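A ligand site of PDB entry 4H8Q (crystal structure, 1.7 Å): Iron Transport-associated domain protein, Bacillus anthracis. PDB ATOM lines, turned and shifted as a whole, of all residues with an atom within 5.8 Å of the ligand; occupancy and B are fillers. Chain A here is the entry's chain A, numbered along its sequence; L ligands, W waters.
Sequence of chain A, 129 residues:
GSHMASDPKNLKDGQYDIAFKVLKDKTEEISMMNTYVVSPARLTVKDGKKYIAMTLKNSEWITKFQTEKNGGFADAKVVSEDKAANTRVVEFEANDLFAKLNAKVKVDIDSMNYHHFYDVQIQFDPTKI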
ATOM      1  N   LEU A  23       6.728  -9.536  -7.317  1.00  0.00           N
ATOM      2  CA  LEU A  23       7.742  -8.864  -8.108  1.00  0.00           C
ATOM      3  C   LEU A  23       9.147  -9.217  -7.646  1.00  0.00           C
ATOM      4  O   LEU A  23       9.398  -9.398  -6.466  1.00  0.00           O
ATOM      5  CB  LEU A  23       7.538  -7.344  -8.023  1.00  0.00           C
ATOM      6  CG  LEU A  23       6.167  -6.819  -8.430  1.00  0.00           C
ATOM      7  CD1 LEU A  23       6.094  -5.311  -8.168  1.00  0.00           C
ATOM      8  CD2 LEU A  23       5.866  -7.154  -9.890  1.00  0.00           C
ATOM      9  N   LYS A  24      10.074  -9.312  -8.596  1.00  0.00           N
ATOM     10  CA  LYS A  24      11.475  -9.484  -8.276  1.00  0.00           C
ATOM     11  C   LYS A  24      11.982  -8.299  -7.455  1.00  0.00           C
ATOM     12  O   LYS A  24      11.613  -7.159  -7.721  1.00  0.00           O
ATOM     13  CB  LYS A  24      12.266  -9.640  -9.585  1.00  0.00           C
ATOM     14  CG  LYS A  24      13.747  -9.761  -9.409  1.00  0.00           C
ATOM     15  CD  LYS A  24      14.414 -10.026 -10.756  1.00  0.00           C
ATOM     16  CE  LYS A  24      15.929 -10.075 -10.631  1.00  0.00           C
ATOM     17  NZ  LYS A  24      16.576 -10.314 -11.940  1.00  0.00           N
ATOM     18  N   ASP A  25      12.806  -8.584  -6.460  1.00  0.00           N
ATOM     19  CA  ASP A  25      13.240  -7.600  -5.464  1.00  0.00           C
ATOM     20  C   ASP A  25      13.743  -6.298  -6.111  1.00  0.00           C
ATOM     21  O   ASP A  25      14.641  -6.336  -6.955  1.00  0.00           O
ATOM     22  CB  ASP A  25      14.345  -8.200  -4.598  1.00  0.00           C
ATOM     23  CG  ASP A  25      14.748  -7.299  -3.431  1.00  0.00           C
ATOM     24  OD1 ASP A  25      13.873  -6.678  -2.809  1.00  0.00           O
ATOM     25  OD2 ASP A  25      15.968  -7.228  -3.145  1.00  0.00           O
ATOM     26  N   ILE A  30       8.170  -9.323 -13.063  1.00  0.00           N
ATOM     27  CA  ILE A  30       7.448 -10.415 -12.416  1.00  0.00           C
ATOM     28  C   ILE A  30       8.420 -11.439 -11.862  1.00  0.00           C
ATOM     29  O   ILE A  30       9.329 -11.891 -12.553  1.00  0.00           O
ATOM     30  CB  ILE A  30       6.450 -11.099 -13.359  1.00  0.00           C
ATOM     31  CG1 ILE A  30       5.480 -10.076 -13.944  1.00  0.00           C
ATOM     32  CG2 ILE A  30       5.670 -12.186 -12.627  1.00  0.00           C
ATOM     33  CD1 ILE A  30       4.713  -9.301 -12.894  1.00  0.00           C
ATOM     34  N   SER A  31       8.220 -11.820 -10.600  1.00  0.00           N
ATOM     35  CA  SER A  31       9.113 -12.765  -9.948  1.00  0.00           C
ATOM     36  C   SER A  31       8.825 -14.188 -10.401  1.00  0.00           C
ATOM     37  O   SER A  31       7.690 -14.524 -10.757  1.00  0.00           O
ATOM     38  CB  SER A  31       8.917 -12.707  -8.427  1.00  0.00           C
ATOM     39  OG  SER A  31       9.737 -13.663  -7.781  1.00  0.00           O
ATOM     40  N   MET A  32       9.861 -15.024 -10.362  1.00  0.00           N
ATOM     41  CA  MET A  32       9.730 -16.476 -10.554  1.00  0.00           C
ATOM     42  C   MET A  32       8.762 -17.041  -9.522  1.00  0.00           C
ATOM     43  O   MET A  32       8.132 -18.081  -9.742  1.00  0.00           O
ATOM     44  CB  MET A  32      11.101 -17.164 -10.404  1.00  0.00           C
ATOM     45  CG  MET A  32      12.067 -16.976 -11.584  1.00  0.00           C
ATOM     46  SD  MET A  32      11.635 -17.901 -13.088  1.00  0.00           S
ATOM     47  CE  MET A  32      11.920 -19.608 -12.596  1.00  0.00           C
ATOM     48  N   MET A  33       8.629 -16.358  -8.391  1.00  0.00           N
ATOM     49  CA  MET A  33       7.704 -16.806  -7.354  1.00  0.00           C
ATOM     50  C   MET A  33       6.253 -16.663  -7.780  1.00  0.00           C
ATOM     51  O   MET A  33       5.381 -17.365  -7.280  1.00  0.00           O
ATOM     52  CB  MET A  33       7.950 -16.074  -6.029  1.00  0.00           C
ATOM     53  CG  MET A  33       6.985 -16.494  -4.939  1.00  0.00           C
ATOM     54  SD  MET A  33       7.550 -15.912  -3.330  1.00  0.00           S
ATOM     55  CE  MET A  33       6.237 -16.606  -2.313  1.00  0.00           C
ATOM     56  N   TYR A  36       4.021 -19.573  -8.395  1.00  0.00           N
ATOM     57  CA  TYR A  36       3.747 -20.500  -7.297  1.00  0.00           C
ATOM     58  C   TYR A  36       2.771 -19.946  -6.271  1.00  0.00           C
ATOM     59  O   TYR A  36       2.662 -20.453  -5.167  1.00  0.00           O
ATOM     60  CB  TYR A  36       5.051 -20.900  -6.603  1.00  0.00           C
ATOM     61  CG  TYR A  36       5.973 -21.645  -7.539  1.00  0.00           C
ATOM     62  CD1 TYR A  36       5.801 -22.996  -7.771  1.00  0.00           C
ATOM     63  CD2 TYR A  36       6.988 -20.984  -8.219  1.00  0.00           C
ATOM     64  CE1 TYR A  36       6.619 -23.682  -8.646  1.00  0.00           C
ATOM     65  CE2 TYR A  36       7.818 -21.652  -9.094  1.00  0.00           C
ATOM     66  CZ  TYR A  36       7.622 -23.011  -9.302  1.00  0.00           C
ATOM     67  OH  TYR A  36       8.433 -23.691 -10.174  1.00  0.00           O
ATOM     68  N   ASN A  58       3.082 -25.852  -4.970  1.00  0.00           N
ATOM     69  CA  ASN A  58       4.302 -26.591  -4.661  1.00  0.00           C
ATOM     70  C   ASN A  58       4.757 -26.361  -3.236  1.00  0.00           C
ATOM     71  O   ASN A  58       5.939 -26.083  -2.969  1.00  0.00           O
ATOM     72  CB  ASN A  58       5.415 -26.233  -5.656  1.00  0.00           C
ATOM     73  CG  ASN A  58       5.162 -26.829  -7.024  1.00  0.00           C
ATOM     74  OD1 ASN A  58       4.564 -26.198  -7.891  1.00  0.00           O
ATOM     75  ND2 ASN A  58       5.591 -28.068  -7.215  1.00  0.00           N
ATOM     76  N   TRP A  61       8.018 -27.442  -1.486  1.00  0.00           N
ATOM     77  CA  TRP A  61       9.261 -26.760  -1.862  1.00  0.00           C
ATOM     78  C   TRP A  61       9.486 -25.444  -1.120  1.00  0.00           C
ATOM     79  O   TRP A  61      10.605 -24.958  -0.999  1.00  0.00           O
ATOM     80  CB  TRP A  61       9.238 -26.438  -3.362  1.00  0.00           C
ATOM     81  CG  TRP A  61       9.389 -27.600  -4.246  1.00  0.00           C
ATOM     82  CD1 TRP A  61       9.703 -28.895  -3.895  1.00  0.00           C
ATOM     83  CD2 TRP A  61       9.233 -27.597  -5.665  1.00  0.00           C
ATOM     84  NE1 TRP A  61       9.754 -29.680  -5.021  1.00  0.00           N
ATOM     85  CE2 TRP A  61       9.454 -28.919  -6.110  1.00  0.00           C
ATOM     86  CE3 TRP A  61       8.910 -26.611  -6.597  1.00  0.00           C
ATOM     87  CZ2 TRP A  61       9.380 -29.261  -7.465  1.00  0.00           C
ATOM     88  CZ3 TRP A  61       8.824 -26.957  -7.940  1.00  0.00           C
ATOM     89  CH2 TRP A  61       9.071 -28.272  -8.359  1.00  0.00           C
ATOM     90  N   ILE A  62       8.400 -24.841  -0.661  1.00  0.00           N
ATOM     91  CA  ILE A  62       8.516 -23.527  -0.031  1.00  0.00           C
ATOM     92  C   ILE A  62       8.643 -23.713   1.464  1.00  0.00           C
ATOM     93  O   ILE A  62       7.669 -24.004   2.139  1.00  0.00           O
ATOM     94  CB  ILE A  62       7.317 -22.622  -0.397  1.00  0.00           C
ATOM     95  CG1 ILE A  62       7.176 -22.535  -1.921  1.00  0.00           C
ATOM     96  CG2 ILE A  62       7.484 -21.246   0.220  1.00  0.00           C
ATOM     97  CD1 ILE A  62       5.903 -21.836  -2.400  1.00  0.00           C
ATOM     98  N   VAL A 105      11.256 -15.424   1.009  1.00  0.00           N
ATOM     99  CA  VAL A 105      10.888 -16.812   0.752  1.00  0.00           C
ATOM    100  C   VAL A 105      12.134 -17.684   0.783  1.00  0.00           C
ATOM    101  O   VAL A 105      13.215 -17.268   0.347  1.00  0.00           O
ATOM    102  CB  VAL A 105      10.128 -16.954  -0.597  1.00  0.00           C
ATOM    103  CG1 VAL A 105      11.034 -16.605  -1.807  1.00  0.00           C
ATOM    104  CG2 VAL A 105       9.520 -18.345  -0.731  1.00  0.00           C
ATOM    105  N   VAL A 107      13.333 -21.551  -0.450  1.00  0.00           N
ATOM    106  CA  VAL A 107      12.919 -22.655  -1.311  1.00  0.00           C
ATOM    107  C   VAL A 107      13.940 -23.796  -1.204  1.00  0.00           C
ATOM    108  O   VAL A 107      15.144 -23.563  -1.224  1.00  0.00           O
ATOM    109  CB  VAL A 107      12.839 -22.210  -2.783  1.00  0.00           C
ATOM    110  CG1 VAL A 107      12.270 -23.317  -3.653  1.00  0.00           C
ATOM    111  CG2 VAL A 107      12.005 -20.931  -2.913  1.00  0.00           C
ATOM    112  N   ILE A 109      14.503 -27.676  -2.910  1.00  0.00           N
ATOM    113  CA  ILE A 109      14.141 -28.803  -3.754  1.00  0.00           C
ATOM    114  C   ILE A 109      15.313 -29.758  -3.738  1.00  0.00           C
ATOM    115  O   ILE A 109      16.271 -29.603  -4.489  1.00  0.00           O
ATOM    116  CB  ILE A 109      13.834 -28.372  -5.201  1.00  0.00           C
ATOM    117  CG1 ILE A 109      12.901 -27.144  -5.213  1.00  0.00           C
ATOM    118  CG2 ILE A 109      13.230 -29.538  -5.967  1.00  0.00           C
ATOM    119  CD1 ILE A 109      12.580 -26.641  -6.576  1.00  0.00           C
ATOM    120  N   MET A 112      16.733 -31.496  -6.971  1.00  0.00           N
ATOM    121  CA  MET A 112      17.263 -30.659  -8.051  1.00  0.00           C
ATOM    122  C   MET A 112      18.396 -29.773  -7.544  1.00  0.00           C
ATOM    123  O   MET A 112      18.820 -28.843  -8.231  1.00  0.00           O
ATOM    124  CB  MET A 112      16.162 -29.814  -8.671  1.00  0.00           C
ATOM    125  CG  MET A 112      15.007 -30.602  -9.265  1.00  0.00           C
ATOM    126  SD  MET A 112      13.642 -29.526  -9.749  1.00  0.00           S
ATOM    127  CE  MET A 112      12.284 -30.706  -9.740  1.00  0.00           C
ATOM    128  N   TYR A 114      18.361 -27.369  -5.441  1.00  0.00           N
ATOM    129  CA  TYR A 114      17.946 -25.974  -5.480  1.00  0.00           C
ATOM    130  C   TYR A 114      17.631 -25.535  -4.063  1.00  0.00           C
ATOM    131  O   TYR A 114      16.633 -25.944  -3.489  1.00  0.00           O
ATOM    132  CB  TYR A 114      16.719 -25.812  -6.374  1.00  0.00           C
ATOM    133  CG  TYR A 114      16.271 -24.386  -6.598  1.00  0.00           C
ATOM    134  CD1 TYR A 114      16.866 -23.591  -7.574  1.00  0.00           C
ATOM    135  CD2 TYR A 114      15.228 -23.842  -5.858  1.00  0.00           C
ATOM    136  CE1 TYR A 114      16.443 -22.291  -7.799  1.00  0.00           C
ATOM    137  CE2 TYR A 114      14.791 -22.546  -6.080  1.00  0.00           C
ATOM    138  CZ  TYR A 114      15.401 -21.771  -7.041  1.00  0.00           C
ATOM    139  OH  TYR A 114      14.947 -20.487  -7.251  1.00  0.00           O
ATOM    140  N   TYR A 118      15.244 -15.652  -0.935  1.00  0.00           N
ATOM    141  CA  TYR A 118      15.099 -14.446  -1.735  1.00  0.00           C
ATOM    142  C   TYR A 118      14.247 -13.427  -1.028  1.00  0.00           C
ATOM    143  O   TYR A 118      13.382 -13.764  -0.216  1.00  0.00           O
ATOM    144  CB  TYR A 118      14.373 -14.754  -3.049  1.00  0.00           C
ATOM    145  CG  TYR A 118      14.995 -15.814  -3.929  1.00  0.00           C
ATOM    146  CD1 TYR A 118      16.062 -15.505  -4.756  1.00  0.00           C
ATOM    147  CD2 TYR A 118      14.480 -17.097  -3.956  1.00  0.00           C
ATOM    148  CE1 TYR A 118      16.622 -16.461  -5.578  1.00  0.00           C
ATOM    149  CE2 TYR A 118      15.051 -18.073  -4.784  1.00  0.00           C
ATOM    150  CZ  TYR A 118      16.107 -17.732  -5.594  1.00  0.00           C
ATOM    151  OH  TYR A 118      16.670 -18.689  -6.407  1.00  0.00           O
ATOM    152  N   ASP A 119      14.474 -12.162  -1.384  1.00  0.00           N
ATOM    153  CA  ASP A 119      13.534 -11.105  -1.107  1.00  0.00           C
ATOM    154  C   ASP A 119      12.614 -10.904  -2.318  1.00  0.00           C
ATOM    155  O   ASP A 119      13.045 -11.040  -3.456  1.00  0.00           O
ATOM    156  CB  ASP A 119      14.289  -9.798  -0.829  1.00  0.00           C
ATOM    157  CG  ASP A 119      15.116  -9.873   0.449  1.00  0.00           C
ATOM    158  OD1 ASP A 119      16.338  -9.629   0.384  1.00  0.00           O
ATOM    159  OD2 ASP A 119      14.542 -10.149   1.515  1.00  0.00           O
ATOM    160  N   VAL A 120      11.341 -10.625  -2.076  1.00  0.00           N
ATOM    161  CA  VAL A 120      10.426 -10.243  -3.142  1.00  0.00           C
ATOM    162  C   VAL A 120       9.488  -9.158  -2.626  1.00  0.00           C
ATOM    163  O   VAL A 120       9.451  -8.877  -1.420  1.00  0.00           O
ATOM    164  CB  VAL A 120       9.540 -11.429  -3.594  1.00  0.00           C
ATOM    165  CG1 VAL A 120      10.384 -12.513  -4.215  1.00  0.00           C
ATOM    166  CG2 VAL A 120       8.754 -11.981  -2.394  1.00  0.00           C
HETATM  167  C1  LIG L   1      15.342 -17.073  -9.243  1.00  0.00           C
HETATM  168  C2  LIG L   1      15.026 -21.417 -11.365  1.00  0.00           C
HETATM  169  C3  LIG L   1      11.592 -22.785  -8.190  1.00  0.00           C
HETATM  170  C4  LIG L   1      11.477 -18.253  -6.437  1.00  0.00           C
HETATM  171  C5  LIG L   1      15.554 -18.131 -10.076  1.00  0.00           C
HETATM  172  C6  LIG L   1      16.522 -18.184 -11.153  1.00  0.00           C
HETATM  173  C7  LIG L   1      16.423 -19.388 -11.732  1.00  0.00           C
HETATM  174  C8  LIG L   1      15.399 -20.140 -11.041  1.00  0.00           C
HETATM  175  C9  LIG L   1      17.245 -19.912 -12.928  1.00  0.00           C
HETATM  176  C10 LIG L   1      17.480 -17.031 -11.565  1.00  0.00           C
HETATM  177  C11 LIG L   1      16.666 -15.897 -12.180  1.00  0.00           C
HETATM  178  C12 LIG L   1      15.895 -16.343 -13.409  1.00  0.00           C
HETATM  179  O1  LIG L   1      16.474 -17.058 -14.268  1.00  0.00           O
HETATM  180  O2  LIG L   1      14.690 -15.985 -13.542  1.00  0.00           O
HETATM  181  C13 LIG L   1      14.058 -22.147 -10.704  1.00  0.00           C
HETATM  182  C14 LIG L   1      13.624 -23.469 -11.083  1.00  0.00           C
HETATM  183  C15 LIG L   1      12.682 -23.850 -10.219  1.00  0.00           C
HETATM  184  C16 LIG L   1      12.486 -22.788  -9.255  1.00  0.00           C
HETATM  185  C17 LIG L   1      14.143 -24.284 -12.291  1.00  0.00           C
HETATM  186  C18 LIG L   1      11.951 -25.217 -10.273  1.00  0.00           C
HETATM  187  C19 LIG L   1      10.936 -25.451  -9.448  1.00  0.00           C
HETATM  188  C20 LIG L   1      11.237 -21.669  -7.463  1.00  0.00           C
HETATM  189  C21 LIG L   1      10.185 -21.597  -6.459  1.00  0.00           C
HETATM  190  C22 LIG L   1      10.149 -20.352  -5.970  1.00  0.00           C
HETATM  191  C23 LIG L   1      11.178 -19.579  -6.649  1.00  0.00           C
HETATM  192  C24 LIG L   1       9.280 -22.786  -6.042  1.00  0.00           C
HETATM  193  C25 LIG L   1       9.190 -19.833  -4.889  1.00  0.00           C
HETATM  194  C26 LIG L   1       9.374 -18.616  -4.388  1.00  0.00           C
HETATM  195  C27 LIG L   1      12.507 -17.552  -7.033  1.00  0.00           C
HETATM  196  C28 LIG L   1      12.820 -16.184  -6.705  1.00  0.00           C
HETATM  197  C29 LIG L   1      14.005 -15.813  -7.569  1.00  0.00           C
HETATM  198  C30 LIG L   1      14.315 -16.995  -8.336  1.00  0.00           C
HETATM  199  C31 LIG L   1      12.089 -15.278  -5.708  1.00  0.00           C
HETATM  200  C32 LIG L   1      14.736 -14.459  -7.610  1.00  0.00           C
HETATM  201  C33 LIG L   1      14.361 -13.712  -8.880  1.00  0.00           C
HETATM  202  C34 LIG L   1      12.887 -13.473  -8.971  1.00  0.00           C
HETATM  203  O3  LIG L   1      12.259 -12.951  -8.002  1.00  0.00           O
HETATM  204  O4  LIG L   1      12.326 -13.804 -10.056  1.00  0.00           O
HETATM  205  N1  LIG L   1      14.890 -19.335 -10.032  1.00  0.00           N
HETATM  206  N2  LIG L   1      13.346 -21.759  -9.579  1.00  0.00           N
HETATM  207  N3  LIG L   1      11.811 -20.416  -7.545  1.00  0.00           N
HETATM  208  N4  LIG L   1      13.411 -18.006  -7.990  1.00  0.00           N
HETATM  209 FE1  LIG L   1      13.523 -19.947  -8.633  1.00  0.00          FE
HETATM  210  O   HOH W   1      13.503 -11.410  -6.110  1.00  0.00           O
HETATM  211  O   HOH W   2      13.499 -14.108 -12.349  1.00  0.00           O
HETATM  212  O   HOH W   3      10.001 -22.324 -11.719  1.00  0.00           O
HETATM  213  O   HOH W   4      16.174 -12.878 -12.282  1.00  0.00           O
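FE1 of the ligand is bound by OH of Tyr 114 (2.1 Å). N of Met 32 lies within hydrogen-bond range of O4 of the ligand (2.8 Å). The side-chain hydroxyl (OG) of Ser 31 lies within hydrogen-bond range of an oxygen (O3) of the ligand (2.6 Å).
The backbone NH of Met 33 sits close to the side-chain hydroxyl of Ser 31. O of Tyr 114 sits at hydrogen-bond distance from N of Ile 109. OH of Tyr 114 lies close to OH of Tyr 118. The backbone NH of Tyr 118 lies within hydrogen-bond range of the backbone carbonyl oxygen of Val 105 (2.9 Å).
Lys 24 touches the ligand. Met 33 touches the ligand (CG to C26, 3.2 Å). Tyr 36 touches the ligand (OH to C19, 3.1 Å). Trp 61 touches the ligand (CZ3 to C19, 3.0 Å). Val 105 touches the ligand. Val 107 touches the ligand. Ile 109 touches the ligand. Tyr 118 touches the ligand (CD1 to C32, 3.3 Å). Val 120 touches the ligand. 12 residues have an atom within 4 Å of the ligand: Lys 24, Ser 31, Met 32, Met 33, Tyr 36, Trp 61, Val 105, Val 107, Ile 109, Tyr 114, Tyr 118 and Val 120. The nearest printed residue that does not touch the ligand is Ile 30 (4.3 Å).
Water W1 lies within hydrogen-bond range of the backbone carbonyl oxygen of Asp 119 (2.7 Å), an oxygen (O3) of the ligand (2.7 Å) and the backbone NH of Asp 25 (2.9 Å).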
